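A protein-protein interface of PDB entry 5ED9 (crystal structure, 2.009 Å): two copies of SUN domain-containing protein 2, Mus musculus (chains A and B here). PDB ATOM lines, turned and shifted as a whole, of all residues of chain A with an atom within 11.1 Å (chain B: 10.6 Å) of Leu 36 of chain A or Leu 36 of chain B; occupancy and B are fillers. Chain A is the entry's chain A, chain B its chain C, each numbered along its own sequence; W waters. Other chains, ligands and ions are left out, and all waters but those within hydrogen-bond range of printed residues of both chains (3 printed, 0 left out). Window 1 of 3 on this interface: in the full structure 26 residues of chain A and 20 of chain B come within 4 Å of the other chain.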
ATOM      1  N   GLN A  28       6.939 -14.063 -17.307  1.00  0.00           N
ATOM      2  CA  GLN A  28       6.378 -15.145 -16.507  1.00  0.00           C
ATOM      3  C   GLN A  28       6.025 -14.656 -15.104  1.00  0.00           C
ATOM      4  O   GLN A  28       4.985 -15.014 -14.550  1.00  0.00           O
ATOM      5  CB  GLN A  28       7.347 -16.333 -16.452  1.00  0.00           C
ATOM      6  CG  GLN A  28       7.482 -17.073 -17.788  1.00  0.00           C
ATOM      7  CD  GLN A  28       8.536 -18.171 -17.772  1.00  0.00           C
ATOM      8  OE1 GLN A  28       9.531 -18.088 -17.051  1.00  0.00           O
ATOM      9  NE2 GLN A  28       8.324 -19.205 -18.579  1.00  0.00           N
ATOM     10  N   LEU A  29       6.900 -13.831 -14.535  1.00  0.00           N
ATOM     11  CA  LEU A  29       6.662 -13.267 -13.217  1.00  0.00           C
ATOM     12  C   LEU A  29       5.434 -12.358 -13.201  1.00  0.00           C
ATOM     13  O   LEU A  29       4.666 -12.364 -12.234  1.00  0.00           O
ATOM     14  CB  LEU A  29       7.899 -12.503 -12.738  1.00  0.00           C
ATOM     15  CG  LEU A  29       9.124 -13.368 -12.433  1.00  0.00           C
ATOM     16  CD1 LEU A  29      10.283 -12.501 -11.933  1.00  0.00           C
ATOM     17  CD2 LEU A  29       8.786 -14.479 -11.435  1.00  0.00           C
ATOM     18  N   ALA A  30       5.254 -11.579 -14.271  1.00  0.00           N
ATOM     19  CA  ALA A  30       4.099 -10.689 -14.397  1.00  0.00           C
ATOM     20  C   ALA A  30       2.794 -11.487 -14.479  1.00  0.00           C
ATOM     21  O   ALA A  30       1.799 -11.133 -13.850  1.00  0.00           O
ATOM     22  CB  ALA A  30       4.244  -9.794 -15.619  1.00  0.00           C
ATOM     23  N   SER A  31       2.805 -12.554 -15.270  1.00  0.00           N
ATOM     24  CA  SER A  31       1.650 -13.442 -15.365  1.00  0.00           C
ATOM     25  C   SER A  31       1.301 -14.069 -14.015  1.00  0.00           C
ATOM     26  O   SER A  31       0.127 -14.157 -13.660  1.00  0.00           O
ATOM     27  CB  SER A  31       1.890 -14.537 -16.400  1.00  0.00           C
ATOM     28  OG  SER A  31       0.713 -15.299 -16.580  1.00  0.00           O
ATOM     29  N   LEU A  32       2.320 -14.495 -13.267  1.00  0.00           N
ATOM     30  CA  LEU A  32       2.119 -15.065 -11.932  1.00  0.00           C
ATOM     31  C   LEU A  32       1.550 -14.054 -10.927  1.00  0.00           C
ATOM     32  O   LEU A  32       0.629 -14.363 -10.173  1.00  0.00           O
ATOM     33  CB  LEU A  32       3.429 -15.637 -11.390  1.00  0.00           C
ATOM     34  CG  LEU A  32       3.281 -16.449 -10.091  1.00  0.00           C
ATOM     35  CD1 LEU A  32       2.427 -17.657 -10.349  1.00  0.00           C
ATOM     36  CD2 LEU A  32       4.625 -16.884  -9.531  1.00  0.00           C
ATOM     37  N   ARG A  33       2.104 -12.844 -10.921  1.00  0.00           N
ATOM     38  CA  ARG A  33       1.648 -11.781 -10.017  1.00  0.00           C
ATOM     39  C   ARG A  33       0.176 -11.448 -10.249  1.00  0.00           C
ATOM     40  O   ARG A  33      -0.568 -11.142  -9.312  1.00  0.00           O
ATOM     41  CB  ARG A  33       2.520 -10.528 -10.203  1.00  0.00           C
ATOM     42  CG  ARG A  33       2.240  -9.368  -9.232  1.00  0.00           C
ATOM     43  CD  ARG A  33       3.415  -8.365  -9.190  1.00  0.00           C
ATOM     44  NE  ARG A  33       3.861  -8.000 -10.533  1.00  0.00           N
ATOM     45  CZ  ARG A  33       5.005  -8.401 -11.077  1.00  0.00           C
ATOM     46  NH1 ARG A  33       5.845  -9.155 -10.379  1.00  0.00           N
ATOM     47  NH2 ARG A  33       5.312  -8.046 -12.318  1.00  0.00           N
ATOM     48  N   GLN A  34      -0.238 -11.498 -11.508  1.00  0.00           N
ATOM     49  CA  GLN A  34      -1.616 -11.199 -11.856  1.00  0.00           C
ATOM     50  C   GLN A  34      -2.555 -12.331 -11.424  1.00  0.00           C
ATOM     51  O   GLN A  34      -3.662 -12.072 -10.955  1.00  0.00           O
ATOM     52  CB  GLN A  34      -1.726 -10.885 -13.349  1.00  0.00           C
ATOM     53  CG  GLN A  34      -1.076  -9.540 -13.705  1.00  0.00           C
ATOM     54  CD  GLN A  34      -0.551  -9.474 -15.131  1.00  0.00           C
ATOM     55  OE1 GLN A  34      -0.867 -10.321 -15.966  1.00  0.00           O
ATOM     56  NE2 GLN A  34       0.275  -8.467 -15.409  1.00  0.00           N
ATOM     57  N   GLU A  35      -2.096 -13.574 -11.569  1.00  0.00           N
ATOM     58  CA  GLU A  35      -2.808 -14.736 -11.042  1.00  0.00           C
ATOM     59  C   GLU A  35      -3.047 -14.619  -9.541  1.00  0.00           C
ATOM     60  O   GLU A  35      -4.152 -14.848  -9.058  1.00  0.00           O
ATOM     61  CB  GLU A  35      -2.021 -16.026 -11.314  1.00  0.00           C
ATOM     62  CG  GLU A  35      -2.132 -16.557 -12.735  1.00  0.00           C
ATOM     63  CD  GLU A  35      -1.577 -17.967 -12.866  1.00  0.00           C
ATOM     64  OE1 GLU A  35      -2.222 -18.919 -12.373  1.00  0.00           O
ATOM     65  OE2 GLU A  35      -0.489 -18.121 -13.449  1.00  0.00           O
ATOM     66  N   LEU A  36      -1.995 -14.291  -8.803  1.00  0.00           N
ATOM     67  CA  LEU A  36      -2.096 -14.107  -7.361  1.00  0.00           C
ATOM     68  C   LEU A  36      -3.123 -13.035  -7.015  1.00  0.00           C
ATOM     69  O   LEU A  36      -3.880 -13.185  -6.062  1.00  0.00           O
ATOM     70  CB  LEU A  36      -0.741 -13.726  -6.763  1.00  0.00           C
ATOM     71  CG  LEU A  36       0.307 -14.834  -6.724  1.00  0.00           C
ATOM     72  CD1 LEU A  36       1.505 -14.411  -5.895  1.00  0.00           C
ATOM     73  CD2 LEU A  36      -0.316 -16.087  -6.166  1.00  0.00           C
ATOM     74  N   ALA A  37      -3.137 -11.956  -7.793  1.00  0.00           N
ATOM     75  CA  ALA A  37      -4.083 -10.863  -7.577  1.00  0.00           C
ATOM     76  C   ALA A  37      -5.510 -11.341  -7.821  1.00  0.00           C
ATOM     77  O   ALA A  37      -6.416 -11.041  -7.042  1.00  0.00           O
ATOM     78  CB  ALA A  37      -3.750  -9.688  -8.490  1.00  0.00           C
ATOM     79  N   ALA A  38      -5.689 -12.095  -8.905  1.00  0.00           N
ATOM     80  CA  ALA A  38      -6.991 -12.630  -9.290  1.00  0.00           C
ATOM     81  C   ALA A  38      -7.542 -13.558  -8.220  1.00  0.00           C
ATOM     82  O   ALA A  38      -8.736 -13.548  -7.927  1.00  0.00           O
ATOM     83  CB  ALA A  38      -6.887 -13.363 -10.624  1.00  0.00           C
ATOM     84  N   LEU A  39      -6.655 -14.357  -7.640  1.00  0.00           N
ATOM     85  CA  LEU A  39      -7.030 -15.313  -6.606  1.00  0.00           C
ATOM     86  C   LEU A  39      -7.424 -14.618  -5.295  1.00  0.00           C
ATOM     87  O   LEU A  39      -8.322 -15.079  -4.591  1.00  0.00           O
ATOM     88  CB  LEU A  39      -5.889 -16.314  -6.384  1.00  0.00           C
ATOM     89  CG  LEU A  39      -6.146 -17.479  -5.427  1.00  0.00           C
ATOM     90  CD1 LEU A  39      -7.258 -18.370  -5.953  1.00  0.00           C
ATOM     91  CD2 LEU A  39      -4.869 -18.276  -5.213  1.00  0.00           C
ATOM     92  N   THR A  40      -6.747 -13.518  -4.968  1.00  0.00           N
ATOM     93  CA  THR A  40      -7.111 -12.697  -3.812  1.00  0.00           C
ATOM     94  C   THR A  40      -8.527 -12.148  -3.971  1.00  0.00           C
ATOM     95  O   THR A  40      -9.305 -12.101  -3.013  1.00  0.00           O
ATOM     96  CB  THR A  40      -6.154 -11.489  -3.634  1.00  0.00           C
ATOM     97  OG1 THR A  40      -4.844 -11.943  -3.288  1.00  0.00           O
ATOM     98  CG2 THR A  40      -6.659 -10.543  -2.540  1.00  0.00           C
ATOM     99  N   LEU A  41      -8.851 -11.734  -5.191  1.00  0.00           N
ATOM    100  CA  LEU A  41     -10.162 -11.199  -5.495  1.00  0.00           C
ATOM    101  C   LEU A  41     -11.250 -12.264  -5.310  1.00  0.00           C
ATOM    102  O   LEU A  41     -12.284 -11.991  -4.707  1.00  0.00           O
ATOM    103  CB  LEU A  41     -10.180 -10.639  -6.916  1.00  0.00           C
ATOM    104  CG  LEU A  41     -11.485  -9.977  -7.364  1.00  0.00           C
ATOM    105  CD1 LEU A  41     -11.986  -8.974  -6.313  1.00  0.00           C
ATOM    106  CD2 LEU A  41     -11.264  -9.282  -8.693  1.00  0.00           C
ATOM    107  N   LYS A  42     -11.018 -13.471  -5.829  1.00  0.00           N
ATOM    108  CA  LYS A  42     -11.950 -14.588  -5.612  1.00  0.00           C
ATOM    109  C   LYS A  42     -12.095 -14.902  -4.130  1.00  0.00           C
ATOM    110  O   LYS A  42     -13.187 -15.162  -3.641  1.00  0.00           O
ATOM    111  CB  LYS A  42     -11.494 -15.844  -6.367  1.00  0.00           C
ATOM    112  CG  LYS A  42     -11.702 -15.776  -7.863  1.00  0.00           C
ATOM    113  CD  LYS A  42     -11.206 -17.038  -8.546  1.00  0.00           C
ATOM    114  CE  LYS A  42     -11.342 -16.935 -10.056  1.00  0.00           C
ATOM    115  NZ  LYS A  42     -12.758 -16.751 -10.479  1.00  0.00           N
ATOM    116  N   GLN A  43     -10.980 -14.866  -3.413  1.00  0.00           N
ATOM    117  CA  GLN A  43     -10.972 -15.156  -1.984  1.00  0.00           C
ATOM    118  C   GLN A  43     -11.859 -14.193  -1.181  1.00  0.00           C
ATOM    119  O   GLN A  43     -12.643 -14.626  -0.337  1.00  0.00           O
ATOM    120  CB  GLN A  43      -9.532 -15.114  -1.472  1.00  0.00           C
ATOM    121  CG  GLN A  43      -9.254 -15.983  -0.271  1.00  0.00           C
ATOM    122  CD  GLN A  43      -7.767 -16.104   0.009  1.00  0.00           C
ATOM    123  OE1 GLN A  43      -7.149 -17.130  -0.275  1.00  0.00           O
ATOM    124  NE2 GLN A  43      -7.188 -15.058   0.571  1.00  0.00           N
ATOM    125  N   ASN A  44     -11.730 -12.893  -1.446  1.00  0.00           N
ATOM    126  CA  ASN A  44     -12.521 -11.877  -0.746  1.00  0.00           C
ATOM    127  C   ASN A  44     -14.011 -11.997  -1.036  1.00  0.00           C
ATOM    128  O   ASN A  44     -14.845 -11.782  -0.159  1.00  0.00           O
ATOM    129  CB  ASN A  44     -12.047 -10.461  -1.112  1.00  0.00           C
ATOM    130  CG  ASN A  44     -10.636 -10.175  -0.633  1.00  0.00           C
ATOM    131  OD1 ASN A  44     -10.137 -10.836   0.277  1.00  0.00           O
ATOM    132  ND2 ASN A  44      -9.990  -9.170  -1.232  1.00  0.00           N
ATOM    133  N   GLN B  28      12.968 -21.403  -8.892  1.00  0.00           N
ATOM    134  CA  GLN B  28      12.090 -20.769  -7.913  1.00  0.00           C
ATOM    135  C   GLN B  28      10.708 -20.530  -8.512  1.00  0.00           C
ATOM    136  O   GLN B  28       9.694 -20.759  -7.851  1.00  0.00           O
ATOM    137  CB  GLN B  28      12.680 -19.452  -7.396  1.00  0.00           C
ATOM    138  CG  GLN B  28      13.879 -19.627  -6.469  1.00  0.00           C
ATOM    139  CD  GLN B  28      14.368 -18.317  -5.893  1.00  0.00           C
ATOM    140  OE1 GLN B  28      13.662 -17.312  -5.935  1.00  0.00           O
ATOM    141  NE2 GLN B  28      15.582 -18.320  -5.349  1.00  0.00           N
ATOM    142  N   LEU B  29      10.671 -20.081  -9.763  1.00  0.00           N
ATOM    143  CA  LEU B  29       9.405 -19.826 -10.435  1.00  0.00           C
ATOM    144  C   LEU B  29       8.575 -21.098 -10.607  1.00  0.00           C
ATOM    145  O   LEU B  29       7.372 -21.091 -10.359  1.00  0.00           O
ATOM    146  CB  LEU B  29       9.635 -19.167 -11.796  1.00  0.00           C
ATOM    147  CG  LEU B  29       8.373 -19.069 -12.660  1.00  0.00           C
ATOM    148  CD1 LEU B  29       7.361 -18.095 -12.063  1.00  0.00           C
ATOM    149  CD2 LEU B  29       8.716 -18.680 -14.079  1.00  0.00           C
ATOM    150  N   ALA B  30       9.222 -22.186 -11.034  1.00  0.00           N
ATOM    151  CA  ALA B  30       8.539 -23.466 -11.222  1.00  0.00           C
ATOM    152  C   ALA B  30       7.932 -23.972  -9.916  1.00  0.00           C
ATOM    153  O   ALA B  30       6.858 -24.568  -9.910  1.00  0.00           O
ATOM    154  CB  ALA B  30       9.491 -24.503 -11.805  1.00  0.00           C
ATOM    155  N   SER B  31       8.627 -23.734  -8.811  1.00  0.00           N
ATOM    156  CA  SER B  31       8.133 -24.158  -7.505  1.00  0.00           C
ATOM    157  C   SER B  31       6.883 -23.363  -7.104  1.00  0.00           C
ATOM    158  O   SER B  31       5.955 -23.920  -6.525  1.00  0.00           O
ATOM    159  CB  SER B  31       9.242 -24.033  -6.453  1.00  0.00           C
ATOM    160  OG  SER B  31       8.756 -24.324  -5.160  1.00  0.00           O
ATOM    161  N   LEU B  32       6.858 -22.073  -7.443  1.00  0.00           N
ATOM    162  CA  LEU B  32       5.699 -21.208  -7.191  1.00  0.00           C
ATOM    163  C   LEU B  32       4.483 -21.567  -8.034  1.00  0.00           C
ATOM    164  O   LEU B  32       3.357 -21.557  -7.541  1.00  0.00           O
ATOM    165  CB  LEU B  32       6.047 -19.739  -7.455  1.00  0.00           C
ATOM    166  CG  LEU B  32       7.033 -19.051  -6.518  1.00  0.00           C
ATOM    167  CD1 LEU B  32       7.205 -17.582  -6.924  1.00  0.00           C
ATOM    168  CD2 LEU B  32       6.546 -19.160  -5.085  1.00  0.00           C
ATOM    169  N   ARG B  33       4.705 -21.853  -9.314  1.00  0.00           N
ATOM    170  CA  ARG B  33       3.610 -22.265 -10.183  1.00  0.00           C
ATOM    171  C   ARG B  33       2.961 -23.561  -9.700  1.00  0.00           C
ATOM    172  O   ARG B  33       1.733 -23.682  -9.707  1.00  0.00           O
ATOM    173  CB  ARG B  33       4.105 -22.447 -11.612  1.00  0.00           C
ATOM    174  CG  ARG B  33       4.479 -21.161 -12.325  1.00  0.00           C
ATOM    175  CD  ARG B  33       4.958 -21.513 -13.722  1.00  0.00           C
ATOM    176  NE  ARG B  33       4.916 -20.387 -14.645  1.00  0.00           N
ATOM    177  CZ  ARG B  33       5.444 -20.413 -15.865  1.00  0.00           C
ATOM    178  NH1 ARG B  33       6.052 -21.508 -16.296  1.00  0.00           N
ATOM    179  NH2 ARG B  33       5.364 -19.343 -16.652  1.00  0.00           N
ATOM    180  N   GLN B  34       3.787 -24.530  -9.302  1.00  0.00           N
ATOM    181  CA  GLN B  34       3.273 -25.792  -8.766  1.00  0.00           C
ATOM    182  C   GLN B  34       2.431 -25.555  -7.511  1.00  0.00           C
ATOM    183  O   GLN B  34       1.344 -26.115  -7.367  1.00  0.00           O
ATOM    184  CB  GLN B  34       4.409 -26.783  -8.489  1.00  0.00           C
ATOM    185  CG  GLN B  34       5.037 -27.412  -9.752  1.00  0.00           C
ATOM    186  CD  GLN B  34       4.184 -28.527 -10.365  1.00  0.00           C
ATOM    187  OE1 GLN B  34       3.093 -28.828  -9.880  1.00  0.00           O
ATOM    188  NE2 GLN B  34       4.693 -29.156 -11.431  1.00  0.00           N
ATOM    189  N   GLU B  35       2.921 -24.711  -6.609  1.00  0.00           N
ATOM    190  CA  GLU B  35       2.183 -24.435  -5.382  1.00  0.00           C
ATOM    191  C   GLU B  35       0.899 -23.650  -5.635  1.00  0.00           C
ATOM    192  O   GLU B  35      -0.140 -23.942  -5.043  1.00  0.00           O
ATOM    193  CB  GLU B  35       3.062 -23.723  -4.347  1.00  0.00           C
ATOM    194  CG  GLU B  35       3.028 -24.405  -2.987  1.00  0.00           C
ATOM    195  CD  GLU B  35       3.701 -23.606  -1.894  1.00  0.00           C
ATOM    196  OE1 GLU B  35       4.949 -23.483  -1.924  1.00  0.00           O
ATOM    197  OE2 GLU B  35       2.978 -23.121  -0.995  1.00  0.00           O
ATOM    198  N   LEU B  36       0.963 -22.656  -6.514  1.00  0.00           N
ATOM    199  CA  LEU B  36      -0.232 -21.895  -6.869  1.00  0.00           C
ATOM    200  C   LEU B  36      -1.293 -22.757  -7.572  1.00  0.00           C
ATOM    201  O   LEU B  36      -2.488 -22.554  -7.382  1.00  0.00           O
ATOM    202  CB  LEU B  36       0.132 -20.696  -7.739  1.00  0.00           C
ATOM    203  CG  LEU B  36      -1.056 -19.840  -8.184  1.00  0.00           C
ATOM    204  CD1 LEU B  36      -1.765 -19.224  -6.984  1.00  0.00           C
ATOM    205  CD2 LEU B  36      -0.609 -18.772  -9.157  1.00  0.00           C
ATOM    206  N   ALA B  37      -0.861 -23.711  -8.388  1.00  0.00           N
ATOM    207  CA  ALA B  37      -1.807 -24.613  -9.043  1.00  0.00           C
ATOM    208  C   ALA B  37      -2.608 -25.400  -8.013  1.00  0.00           C
ATOM    209  O   ALA B  37      -3.834 -25.506  -8.115  1.00  0.00           O
ATOM    210  CB  ALA B  37      -1.081 -25.561  -9.996  1.00  0.00           C
ATOM    211  N   ALA B  38      -1.916 -25.939  -7.013  1.00  0.00           N
ATOM    212  CA  ALA B  38      -2.576 -26.673  -5.933  1.00  0.00           C
ATOM    213  C   ALA B  38      -3.524 -25.780  -5.130  1.00  0.00           C
ATOM    214  O   ALA B  38      -4.615 -26.203  -4.733  1.00  0.00           O
ATOM    215  CB  ALA B  38      -1.544 -27.310  -5.014  1.00  0.00           C
ATOM    216  N   LEU B  39      -3.113 -24.540  -4.897  1.00  0.00           N
ATOM    217  CA  LEU B  39      -3.933 -23.624  -4.106  1.00  0.00           C
ATOM    218  C   LEU B  39      -5.189 -23.186  -4.851  1.00  0.00           C
ATOM    219  O   LEU B  39      -6.255 -23.052  -4.252  1.00  0.00           O
ATOM    220  CB  LEU B  39      -3.127 -22.401  -3.696  1.00  0.00           C
ATOM    221  CG  LEU B  39      -3.813 -21.507  -2.668  1.00  0.00           C
ATOM    222  CD1 LEU B  39      -4.067 -22.263  -1.364  1.00  0.00           C
ATOM    223  CD2 LEU B  39      -2.979 -20.246  -2.418  1.00  0.00           C
ATOM    224  N   THR B  40      -5.043 -22.945  -6.153  1.00  0.00           N
ATOM    225  CA  THR B  40      -6.158 -22.552  -7.006  1.00  0.00           C
ATOM    226  C   THR B  40      -7.295 -23.579  -6.939  1.00  0.00           C
ATOM    227  O   THR B  40      -8.460 -23.218  -6.773  1.00  0.00           O
ATOM    228  CB  THR B  40      -5.692 -22.368  -8.471  1.00  0.00           C
ATOM    229  OG1 THR B  40      -4.708 -21.325  -8.541  1.00  0.00           O
ATOM    230  CG2 THR B  40      -6.865 -22.008  -9.373  1.00  0.00           C
ATOM    231  N   LEU B  41      -6.943 -24.858  -7.068  1.00  0.00           N
ATOM    232  CA  LEU B  41      -7.900 -25.954  -6.957  1.00  0.00           C
ATOM    233  C   LEU B  41      -8.600 -25.963  -5.602  1.00  0.00           C
ATOM    234  O   LEU B  41      -9.818 -26.126  -5.524  1.00  0.00           O
ATOM    235  CB  LEU B  41      -7.191 -27.291  -7.181  1.00  0.00           C
ATOM    236  CG  LEU B  41      -6.761 -27.578  -8.619  1.00  0.00           C
ATOM    237  CD1 LEU B  41      -5.947 -28.859  -8.679  1.00  0.00           C
ATOM    238  CD2 LEU B  41      -7.963 -27.669  -9.552  1.00  0.00           C
ATOM    239  N   LYS B  42      -7.825 -25.809  -4.533  1.00  0.00           N
ATOM    240  CA  LYS B  42      -8.385 -25.778  -3.184  1.00  0.00           C
ATOM    241  C   LYS B  42      -9.369 -24.623  -3.031  1.00  0.00           C
ATOM    242  O   LYS B  42     -10.449 -24.775  -2.455  1.00  0.00           O
ATOM    243  CB  LYS B  42      -7.274 -25.647  -2.137  1.00  0.00           C
ATOM    244  CG  LYS B  42      -6.541 -26.943  -1.841  1.00  0.00           C
ATOM    245  CD  LYS B  42      -5.725 -26.819  -0.562  1.00  0.00           C
ATOM    246  CE  LYS B  42      -5.530 -28.183   0.095  1.00  0.00           C
ATOM    247  NZ  LYS B  42      -4.697 -28.108   1.335  1.00  0.00           N
ATOM    248  N   GLN B  43      -8.985 -23.466  -3.545  1.00  0.00           N
ATOM    249  CA  GLN B  43      -9.828 -22.288  -3.435  1.00  0.00           C
ATOM    250  C   GLN B  43     -11.104 -22.452  -4.256  1.00  0.00           C
ATOM    251  O   GLN B  43     -12.184 -22.059  -3.814  1.00  0.00           O
ATOM    252  CB  GLN B  43      -9.063 -21.048  -3.893  1.00  0.00           C
ATOM    253  CG  GLN B  43      -9.667 -19.751  -3.402  1.00  0.00           C
ATOM    254  CD  GLN B  43     -10.863 -19.329  -4.211  1.00  0.00           C
ATOM    255  OE1 GLN B  43     -10.914 -19.559  -5.421  1.00  0.00           O
ATOM    256  NE2 GLN B  43     -11.845 -18.712  -3.551  1.00  0.00           N
ATOM    257  N   ASN B  44     -10.967 -23.015  -5.455  1.00  0.00           N
ATOM    258  CA  ASN B  44     -12.108 -23.278  -6.324  1.00  0.00           C
ATOM    259  C   ASN B  44     -13.099 -24.222  -5.658  1.00  0.00           C
ATOM    260  O   ASN B  44     -14.305 -24.056  -5.796  1.00  0.00           O
ATOM    261  CB  ASN B  44     -11.650 -23.885  -7.654  1.00  0.00           C
ATOM    262  CG  ASN B  44     -11.098 -22.850  -8.616  1.00  0.00           C
ATOM    263  OD1 ASN B  44     -11.061 -21.660  -8.316  1.00  0.00           O
ATOM    264  ND2 ASN B  44     -10.664 -23.302  -9.781  1.00  0.00           N
HETATM  265  O   HOH W   1      -4.714 -19.171 -10.291  1.00  0.00           O
HETATM  266  O   HOH W   2       3.846 -17.666 -14.730  1.00  0.00           O
HETATM  267  O   HOH W   3      -2.111 -21.699 -10.912  1.00  0.00           O
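Water W1 bridges OG1 of Thr 40 of chain B and OE1 of Glu 35 of chain A.
Water W2 bridges O of Gln 28 of chain A and NE of Arg 33 of chain B.
Water W3 bridges the side-chain carboxylate (OE1) of Glu 35 of chain A and the backbone NH (N) of Ala 37 of chain B.
Among the printed residues, merely in contact across the chains: Gln 28 of chain A with Leu 29 of chain B (3.1 Å), Gln 28 of chain A with Arg 33 of chain B (3.3 Å), Leu 32 of chain A with Leu 36 of chain B (3.4 Å), Leu 36 of chain A with Leu 36 of chain B (3.6 Å), Glu 35 of chain A with Leu 36 of chain B (3.6 Å), Leu 39 of chain A with Leu 36 of chain B (3.7 Å), Leu 32 of chain A with Leu 32 of chain B (3.7 Å), Leu 39 of chain A with Gln 43 of chain B (3.8 Å), Lys 42 of chain A with Gln 43 of chain B (3.8 Å), Leu 39 of chain A with Leu 39 of chain B (3.9 Å), Leu 32 of chain A with Leu 29 of chain B (3.9 Å), Leu 29 of chain A with Leu 29 of chain B (3.9 Å) and Gln 43 of chain A with Gln 43 of chain B (3.9 Å).
Of the printed residues of chain B, Gln 28 of chain A touches Leu 29 (3.1 Å) and Arg 33 (3.3 Å).
Of the printed residues of chain B, Leu 32 of chain A touches Leu 29, Leu 32 and Leu 36.
Of the printed residues of chain B, Glu 35 of chain A touches Leu 36 (3.6 Å).
No residue of chain B comes within 4 Å of Ala 38 of chain A.
Of the printed residues of chain B, Lys 42 of chain A touches Gln 43.
Of the printed residues of chain B, Gln 43 of chain A touches Gln 43 (3.9 Å).
Ala 30 of chain B touches none of the printed residues of chain A.
No residue of chain A comes within 4 Å of Glu 35 of chain B.
Of chain A, only Leu 32 (3.4 Å), Glu 35 (3.6 Å), Leu 36 (3.6 Å) and Leu 39 (3.7 Å) come within 4 Å of Leu 36 of chain B.
No residue of chain A comes within 4 Å of Ala 38 of chain B.
Of chain A, only Leu 39 (3.9 Å) comes within 4 Å of Leu 39 of chain B.
Printed residues of chain A within 4 Å of Gln 43 of chain B: Leu 39 (3.8 Å), Lys 42 (3.8 Å) and Gln 43 (3.9 Å).
Asn 44 of chain B touches none of the printed residues of chain A.
The nearest residue of chain B that does not touch Leu 36 of chain A is Leu 39 of chain B (6.2 Å).
The nearest residue of chain A that does not touch Leu 36 of chain B is Ser 31 of chain A (6.5 Å).
The nearest printed residue of chain B that does not touch Gln 43 of chain A is Leu 39 of chain B (5.6 Å).
Of the 17 printed residues of chain A, 8 touch a printed residue of chain B.
Hydrophobic or aromatic side chains of chain A within 4 Å of the printed part of chain B: Leu 29, Leu 32, Leu 36 and Leu 39.
Along chain A the printed residues that touch a printed residue of chain B span positions 28 to 43.
Hydrophobic or aromatic side chains of chain B within 4 Å of the printed part of chain A: Leu 29, Leu 32, Leu 36 and Leu 39.
Along chain B the printed residues that touch a printed residue of chain A span positions 29 to 43.
Among the printed residues, 13 pairs touch across the chains.
Among the printed residues, no Asp or Glu carboxylate lies within 4 Å of a Lys or Arg side-chain nitrogen of the other chain.
Gln 28 of chain A touches Arg 33 of chain B, but with the chains exchanged Arg 33 of chain A does not touch Gln 28 of chain B (11.4 Å).
Glu 35 of chain A touches Leu 36 of chain B, but with the chains exchanged Leu 36 of chain A does not touch Glu 35 of chain B (7.7 Å).
Leu 36 of chain A touches its own counterpart, Leu 36 of chain B.
Leu 39 of chain A touches Leu 36 of chain B, but with the chains exchanged Leu 36 of chain A does not touch Leu 39 of chain B (6.2 Å).
Positions printed for both chains: 28, 29, 30, 31, 32, 33, 34, 35, 36, 37, 38, 39, 40, 41, 42, 43 and 44.
Of the 13 pairs that touch across the chains among the printed residues, 5 have their exchanged pair printed and touching as well.
The side-chain hydroxyl of Thr 40 of chain A is in hydrogen-bond range of the backbone carbonyl oxygen of Leu 36 of chain A (3.2 Å).
O of Leu 36 of chain B lies within hydrogen-bond range of OG1 of Thr 40 of chain B, at 2.8 Å.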
